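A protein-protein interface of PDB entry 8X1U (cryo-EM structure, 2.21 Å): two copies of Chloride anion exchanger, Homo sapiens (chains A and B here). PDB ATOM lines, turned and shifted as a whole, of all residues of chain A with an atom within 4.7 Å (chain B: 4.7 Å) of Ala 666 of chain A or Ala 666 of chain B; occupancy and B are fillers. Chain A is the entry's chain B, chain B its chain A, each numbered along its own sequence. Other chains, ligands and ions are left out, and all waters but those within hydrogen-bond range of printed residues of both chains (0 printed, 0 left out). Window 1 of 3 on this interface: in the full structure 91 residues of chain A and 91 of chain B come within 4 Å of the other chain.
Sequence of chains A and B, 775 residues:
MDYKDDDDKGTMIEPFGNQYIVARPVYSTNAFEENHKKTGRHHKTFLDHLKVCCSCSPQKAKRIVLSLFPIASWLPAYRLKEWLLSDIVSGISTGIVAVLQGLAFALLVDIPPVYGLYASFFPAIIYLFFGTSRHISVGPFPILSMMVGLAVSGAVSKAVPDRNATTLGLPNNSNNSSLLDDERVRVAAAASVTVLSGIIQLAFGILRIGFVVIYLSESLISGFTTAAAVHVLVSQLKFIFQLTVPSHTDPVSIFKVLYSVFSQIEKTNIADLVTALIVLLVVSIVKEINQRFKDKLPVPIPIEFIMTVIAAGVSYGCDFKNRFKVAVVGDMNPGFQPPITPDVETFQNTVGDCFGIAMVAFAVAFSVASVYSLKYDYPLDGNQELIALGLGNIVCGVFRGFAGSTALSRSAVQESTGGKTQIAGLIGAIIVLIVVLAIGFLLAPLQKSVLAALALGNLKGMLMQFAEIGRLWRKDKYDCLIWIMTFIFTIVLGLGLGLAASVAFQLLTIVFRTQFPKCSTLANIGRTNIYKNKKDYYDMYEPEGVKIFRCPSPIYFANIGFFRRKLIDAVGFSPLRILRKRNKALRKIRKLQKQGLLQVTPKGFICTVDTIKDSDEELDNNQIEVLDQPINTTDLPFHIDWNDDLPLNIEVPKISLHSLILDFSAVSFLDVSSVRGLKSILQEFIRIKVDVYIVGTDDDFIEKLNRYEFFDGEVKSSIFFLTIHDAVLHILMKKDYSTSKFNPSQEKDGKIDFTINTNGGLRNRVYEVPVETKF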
ATOM      1  N   ARG A 550     -20.842 -19.423  26.031  1.00  0.00           N
ATOM      2  CA  ARG A 550     -20.611 -20.749  25.480  1.00  0.00           C
ATOM      3  C   ARG A 550     -21.579 -21.002  24.336  1.00  0.00           C
ATOM      4  O   ARG A 550     -22.794 -20.906  24.514  1.00  0.00           O
ATOM      5  CB  ARG A 550     -20.769 -21.814  26.562  1.00  0.00           C
ATOM      6  CG  ARG A 550     -20.710 -23.222  26.038  1.00  0.00           C
ATOM      7  CD  ARG A 550     -20.988 -24.230  27.122  1.00  0.00           C
ATOM      8  NE  ARG A 550     -21.301 -25.535  26.557  1.00  0.00           N
ATOM      9  CZ  ARG A 550     -20.390 -26.447  26.239  1.00  0.00           C
ATOM     10  NH1 ARG A 550     -20.767 -27.607  25.730  1.00  0.00           N
ATOM     11  NH2 ARG A 550     -19.106 -26.199  26.433  1.00  0.00           N
ATOM     12  N   CYS A 551     -21.037 -21.304  23.158  1.00  0.00           N
ATOM     13  CA  CYS A 551     -21.814 -21.837  22.049  1.00  0.00           C
ATOM     14  C   CYS A 551     -21.495 -23.316  21.914  1.00  0.00           C
ATOM     15  O   CYS A 551     -20.339 -23.666  21.632  1.00  0.00           O
ATOM     16  CB  CYS A 551     -21.502 -21.103  20.749  1.00  0.00           C
ATOM     17  SG  CYS A 551     -22.457 -21.673  19.322  1.00  0.00           S
ATOM     18  N   PRO A 552     -22.475 -24.180  22.199  1.00  0.00           N
ATOM     19  CA  PRO A 552     -22.335 -25.633  22.247  1.00  0.00           C
ATOM     20  C   PRO A 552     -22.323 -26.404  20.947  1.00  0.00           C
ATOM     21  O   PRO A 552     -22.856 -27.504  20.932  1.00  0.00           O
ATOM     22  CB  PRO A 552     -23.545 -26.051  23.067  1.00  0.00           C
ATOM     23  CG  PRO A 552     -24.568 -25.036  22.740  1.00  0.00           C
ATOM     24  CD  PRO A 552     -23.846 -23.752  22.502  1.00  0.00           C
ATOM     25  N   SER A 553     -21.838 -25.783  19.871  1.00  0.00           N
ATOM     26  CA  SER A 553     -21.858 -26.398  18.552  1.00  0.00           C
ATOM     27  C   SER A 553     -20.815 -25.819  17.627  1.00  0.00           C
ATOM     28  O   SER A 553     -20.242 -24.777  17.916  1.00  0.00           O
ATOM     29  CB  SER A 553     -23.221 -26.166  17.900  1.00  0.00           C
ATOM     30  OG  SER A 553     -23.342 -24.849  17.400  1.00  0.00           O
ATOM     31  N   PRO A 554     -20.561 -26.491  16.496  1.00  0.00           N
ATOM     32  CA  PRO A 554     -19.656 -25.888  15.515  1.00  0.00           C
ATOM     33  C   PRO A 554     -20.261 -24.599  14.975  1.00  0.00           C
ATOM     34  O   PRO A 554     -21.470 -24.517  14.820  1.00  0.00           O
ATOM     35  CB  PRO A 554     -19.604 -26.929  14.399  1.00  0.00           C
ATOM     36  CG  PRO A 554     -20.012 -28.210  15.043  1.00  0.00           C
ATOM     37  CD  PRO A 554     -21.010 -27.831  16.090  1.00  0.00           C
ATOM     38  N   PHE A 664     -14.998 -22.072  23.764  1.00  0.00           N
ATOM     39  CA  PHE A 664     -15.025 -22.741  22.471  1.00  0.00           C
ATOM     40  C   PHE A 664     -14.749 -24.234  22.592  1.00  0.00           C
ATOM     41  O   PHE A 664     -14.221 -24.843  21.657  1.00  0.00           O
ATOM     42  CB  PHE A 664     -14.018 -22.086  21.527  1.00  0.00           C
ATOM     43  CG  PHE A 664     -14.595 -20.990  20.681  1.00  0.00           C
ATOM     44  CD1 PHE A 664     -15.663 -20.236  21.125  1.00  0.00           C
ATOM     45  CD2 PHE A 664     -14.064 -20.712  19.437  1.00  0.00           C
ATOM     46  CE1 PHE A 664     -16.190 -19.236  20.347  1.00  0.00           C
ATOM     47  CE2 PHE A 664     -14.589 -19.712  18.658  1.00  0.00           C
ATOM     48  CZ  PHE A 664     -15.654 -18.973  19.115  1.00  0.00           C
ATOM     49  N   SER A 665     -15.059 -24.854  23.718  1.00  0.00           N
ATOM     50  CA  SER A 665     -14.769 -26.280  23.864  1.00  0.00           C
ATOM     51  C   SER A 665     -15.576 -27.195  22.946  1.00  0.00           C
ATOM     52  O   SER A 665     -15.059 -28.169  22.430  1.00  0.00           O
ATOM     53  CB  SER A 665     -14.880 -26.735  25.315  1.00  0.00           C
ATOM     54  OG  SER A 665     -16.215 -26.757  25.748  1.00  0.00           O
ATOM     55  N   ALA A 666     -16.846 -26.888  22.748  1.00  0.00           N
ATOM     56  CA  ALA A 666     -17.659 -27.710  21.864  1.00  0.00           C
ATOM     57  C   ALA A 666     -17.760 -27.154  20.455  1.00  0.00           C
ATOM     58  O   ALA A 666     -18.526 -27.690  19.653  1.00  0.00           O
ATOM     59  CB  ALA A 666     -19.062 -27.880  22.445  1.00  0.00           C
ATOM     60  N   VAL A 667     -17.019 -26.097  20.132  1.00  0.00           N
ATOM     61  CA  VAL A 667     -16.961 -25.578  18.768  1.00  0.00           C
ATOM     62  C   VAL A 667     -15.959 -26.446  18.013  1.00  0.00           C
ATOM     63  O   VAL A 667     -14.749 -26.265  18.128  1.00  0.00           O
ATOM     64  CB  VAL A 667     -16.578 -24.098  18.728  1.00  0.00           C
ATOM     65  CG1 VAL A 667     -16.380 -23.637  17.301  1.00  0.00           C
ATOM     66  CG2 VAL A 667     -17.643 -23.263  19.402  1.00  0.00           C
ATOM     67  N   SER A 668     -16.470 -27.404  17.242  1.00  0.00           N
ATOM     68  CA  SER A 668     -15.614 -28.384  16.586  1.00  0.00           C
ATOM     69  C   SER A 668     -14.831 -27.764  15.435  1.00  0.00           C
ATOM     70  O   SER A 668     -13.619 -27.957  15.320  1.00  0.00           O
ATOM     71  CB  SER A 668     -16.455 -29.560  16.091  1.00  0.00           C
ATOM     72  OG  SER A 668     -17.365 -29.978  17.091  1.00  0.00           O
ATOM     73  N   ARG B 550     -10.213 -38.931  22.551  1.00  0.00           N
ATOM     74  CA  ARG B 550     -10.904 -37.698  22.206  1.00  0.00           C
ATOM     75  C   ARG B 550     -11.308 -37.727  20.741  1.00  0.00           C
ATOM     76  O   ARG B 550     -10.465 -37.931  19.862  1.00  0.00           O
ATOM     77  CB  ARG B 550     -10.022 -36.483  22.491  1.00  0.00           C
ATOM     78  CG  ARG B 550     -10.395 -35.265  21.688  1.00  0.00           C
ATOM     79  CD  ARG B 550      -9.605 -34.050  22.115  1.00  0.00           C
ATOM     80  NE  ARG B 550     -10.105 -32.838  21.482  1.00  0.00           N
ATOM     81  CZ  ARG B 550     -11.004 -32.032  22.031  1.00  0.00           C
ATOM     82  NH1 ARG B 550     -11.411 -30.951  21.387  1.00  0.00           N
ATOM     83  NH2 ARG B 550     -11.500 -32.312  23.225  1.00  0.00           N
ATOM     84  N   CYS B 551     -12.602 -37.537  20.485  1.00  0.00           N
ATOM     85  CA  CYS B 551     -13.125 -37.270  19.154  1.00  0.00           C
ATOM     86  C   CYS B 551     -13.535 -35.808  19.090  1.00  0.00           C
ATOM     87  O   CYS B 551     -14.426 -35.392  19.846  1.00  0.00           O
ATOM     88  CB  CYS B 551     -14.314 -38.171  18.834  1.00  0.00           C
ATOM     89  SG  CYS B 551     -15.016 -37.920  17.190  1.00  0.00           S
ATOM     90  N   PRO B 552     -12.910 -34.990  18.246  1.00  0.00           N
ATOM     91  CA  PRO B 552     -13.154 -33.545  18.252  1.00  0.00           C
ATOM     92  C   PRO B 552     -14.274 -33.097  17.316  1.00  0.00           C
ATOM     93  O   PRO B 552     -14.126 -32.132  16.561  1.00  0.00           O
ATOM     94  CB  PRO B 552     -11.805 -32.984  17.803  1.00  0.00           C
ATOM     95  CG  PRO B 552     -11.326 -34.013  16.828  1.00  0.00           C
ATOM     96  CD  PRO B 552     -11.861 -35.352  17.281  1.00  0.00           C
ATOM     97  N   SER B 553     -15.378 -33.823  17.364  1.00  0.00           N
ATOM     98  CA  SER B 553     -16.483 -33.580  16.466  1.00  0.00           C
ATOM     99  C   SER B 553     -17.789 -34.183  16.965  1.00  0.00           C
ATOM    100  O   SER B 553     -17.776 -35.078  17.784  1.00  0.00           O
ATOM    101  CB  SER B 553     -16.094 -34.245  15.141  1.00  0.00           C
ATOM    102  OG  SER B 553     -17.038 -34.091  14.119  1.00  0.00           O
ATOM    103  N   PRO B 554     -18.937 -33.674  16.486  1.00  0.00           N
ATOM    104  CA  PRO B 554     -20.194 -34.331  16.845  1.00  0.00           C
ATOM    105  C   PRO B 554     -20.236 -35.719  16.233  1.00  0.00           C
ATOM    106  O   PRO B 554     -19.762 -35.904  15.121  1.00  0.00           O
ATOM    107  CB  PRO B 554     -21.254 -33.447  16.195  1.00  0.00           C
ATOM    108  CG  PRO B 554     -20.583 -32.145  15.927  1.00  0.00           C
ATOM    109  CD  PRO B 554     -19.148 -32.473  15.665  1.00  0.00           C
ATOM    110  N   PHE B 664     -15.624 -36.286  25.696  1.00  0.00           N
ATOM    111  CA  PHE B 664     -16.758 -35.889  24.872  1.00  0.00           C
ATOM    112  C   PHE B 664     -17.005 -34.387  24.925  1.00  0.00           C
ATOM    113  O   PHE B 664     -18.142 -33.941  24.757  1.00  0.00           O
ATOM    114  CB  PHE B 664     -18.013 -36.643  25.307  1.00  0.00           C
ATOM    115  CG  PHE B 664     -18.286 -37.886  24.515  1.00  0.00           C
ATOM    116  CD1 PHE B 664     -17.253 -38.670  24.044  1.00  0.00           C
ATOM    117  CD2 PHE B 664     -19.583 -38.273  24.248  1.00  0.00           C
ATOM    118  CE1 PHE B 664     -17.512 -39.810  23.322  1.00  0.00           C
ATOM    119  CE2 PHE B 664     -19.842 -39.411  23.528  1.00  0.00           C
ATOM    120  CZ  PHE B 664     -18.806 -40.179  23.065  1.00  0.00           C
ATOM    121  N   SER B 665     -15.955 -33.599  25.153  1.00  0.00           N
ATOM    122  CA  SER B 665     -16.123 -32.164  25.340  1.00  0.00           C
ATOM    123  C   SER B 665     -16.505 -31.468  24.042  1.00  0.00           C
ATOM    124  O   SER B 665     -17.422 -30.639  24.026  1.00  0.00           O
ATOM    125  CB  SER B 665     -14.847 -31.561  25.913  1.00  0.00           C
ATOM    126  OG  SER B 665     -13.918 -31.285  24.884  1.00  0.00           O
ATOM    127  N   ALA B 666     -15.818 -31.783  22.949  1.00  0.00           N
ATOM    128  CA  ALA B 666     -16.099 -31.172  21.659  1.00  0.00           C
ATOM    129  C   ALA B 666     -17.146 -31.926  20.861  1.00  0.00           C
ATOM    130  O   ALA B 666     -17.417 -31.553  19.719  1.00  0.00           O
ATOM    131  CB  ALA B 666     -14.818 -31.055  20.832  1.00  0.00           C
ATOM    132  N   VAL B 667     -17.736 -32.976  21.425  1.00  0.00           N
ATOM    133  CA  VAL B 667     -18.808 -33.714  20.763  1.00  0.00           C
ATOM    134  C   VAL B 667     -20.094 -32.928  20.991  1.00  0.00           C
ATOM    135  O   VAL B 667     -20.639 -32.908  22.092  1.00  0.00           O
ATOM    136  CB  VAL B 667     -18.920 -35.150  21.272  1.00  0.00           C
ATOM    137  CG1 VAL B 667     -20.152 -35.802  20.711  1.00  0.00           C
ATOM    138  CG2 VAL B 667     -17.688 -35.936  20.884  1.00  0.00           C
ATOM    139  N   SER B 668     -20.580 -32.274  19.938  1.00  0.00           N
ATOM    140  CA  SER B 668     -21.714 -31.367  20.062  1.00  0.00           C
ATOM    141  C   SER B 668     -23.021 -32.125  20.260  1.00  0.00           C
ATOM    142  O   SER B 668     -23.699 -31.957  21.278  1.00  0.00           O
ATOM    143  CB  SER B 668     -21.792 -30.471  18.828  1.00  0.00           C
ATOM    144  OG  SER B 668     -20.685 -29.593  18.786  1.00  0.00           O
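O of Ala 666 of chain B sits at hydrogen-bond distance from OG of Ser 668 of chain A (3.1 Å). The side-chain hydroxyl (OG) of Ser 668 of chain B is in hydrogen-bond range of the backbone carbonyl oxygen (O) of Ala 666 of chain A, 3.0 Å away.
The guanidinium group of Arg 550 of chain B sits at hydrogen-bond distance from the side-chain hydroxyl of Ser 665 of chain B. The guanidinium group of Arg 550 of chain A is in hydrogen-bond range of the side-chain hydroxyl of Ser 665 of chain A (3.0 Å).
Among the printed residues, pairs that only touch across the chains: Pro 554 of chain A with Ser 668 of chain B (3.2 Å), Ser 665 of chain A with Ala 666 of chain B (3.3 Å), Ser 668 of chain A with Pro 554 of chain B (3.4 Å), Ser 553 of chain A with Ser 668 of chain B (3.4 Å), Ser 668 of chain A with Pro 552 of chain B (3.5 Å), Ala 666 of chain A with Ser 665 of chain B (3.6 Å), Pro 552 of chain A with Ser 668 of chain B (3.7 Å), Ser 668 of chain A with Ser 668 of chain B (3.7 Å), Ser 668 of chain A with Ser 553 of chain B (3.8 Å), Ser 665 of chain A with Ser 665 of chain B (3.8 Å) and Ala 666 of chain A with Ala 666 of chain B (3.8 Å).
Ala 666 of chain B touches three residues of chain A. Of the printed residues of chain B, Pro 554 of chain A touches Ser 668 (3.2 Å). Of the printed residues of chain B, Ser 668 of chain A touches Pro 552, Ser 553, Pro 554, Ala 666 and Ser 668. Phe 664 of chain A touches none of the printed residues of chain B. The nearest printed residue of chain B that does not touch Ser 553 of chain A is Pro 554 of chain B (6.4 Å).
Of the 10 printed residues of chain B, 6 touch a printed residue of chain A. Hydrophobic or aromatic side chains of chain B within 4 Å of the printed part of chain A: Pro 554 and Ala 666. Among the printed residues, 13 pairs touch across the chains. Among the printed residues, no Asp or Glu carboxylate lies within 4 Å of a Lys or Arg side-chain nitrogen of the other chain.
Ser 553 of chain A touches Ser 668 of chain B, and with the chains exchanged Ser 668 of chain A touches Ser 553 of chain B. Pro 554 of chain A touches Ser 668 of chain B, and with the chains exchanged Ser 668 of chain A touches Pro 554 of chain B. Ala 666 of chain A touches Ser 668 of chain B, and with the chains exchanged Ser 668 of chain A touches Ala 666 of chain B. Ser 668 of chain B touches its own counterpart, Ser 668 of chain A. 10 positions are printed for both chains. Of the 13 pairs that touch across the chains among the printed residues, 13 have their exchanged pair printed and touching as well.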
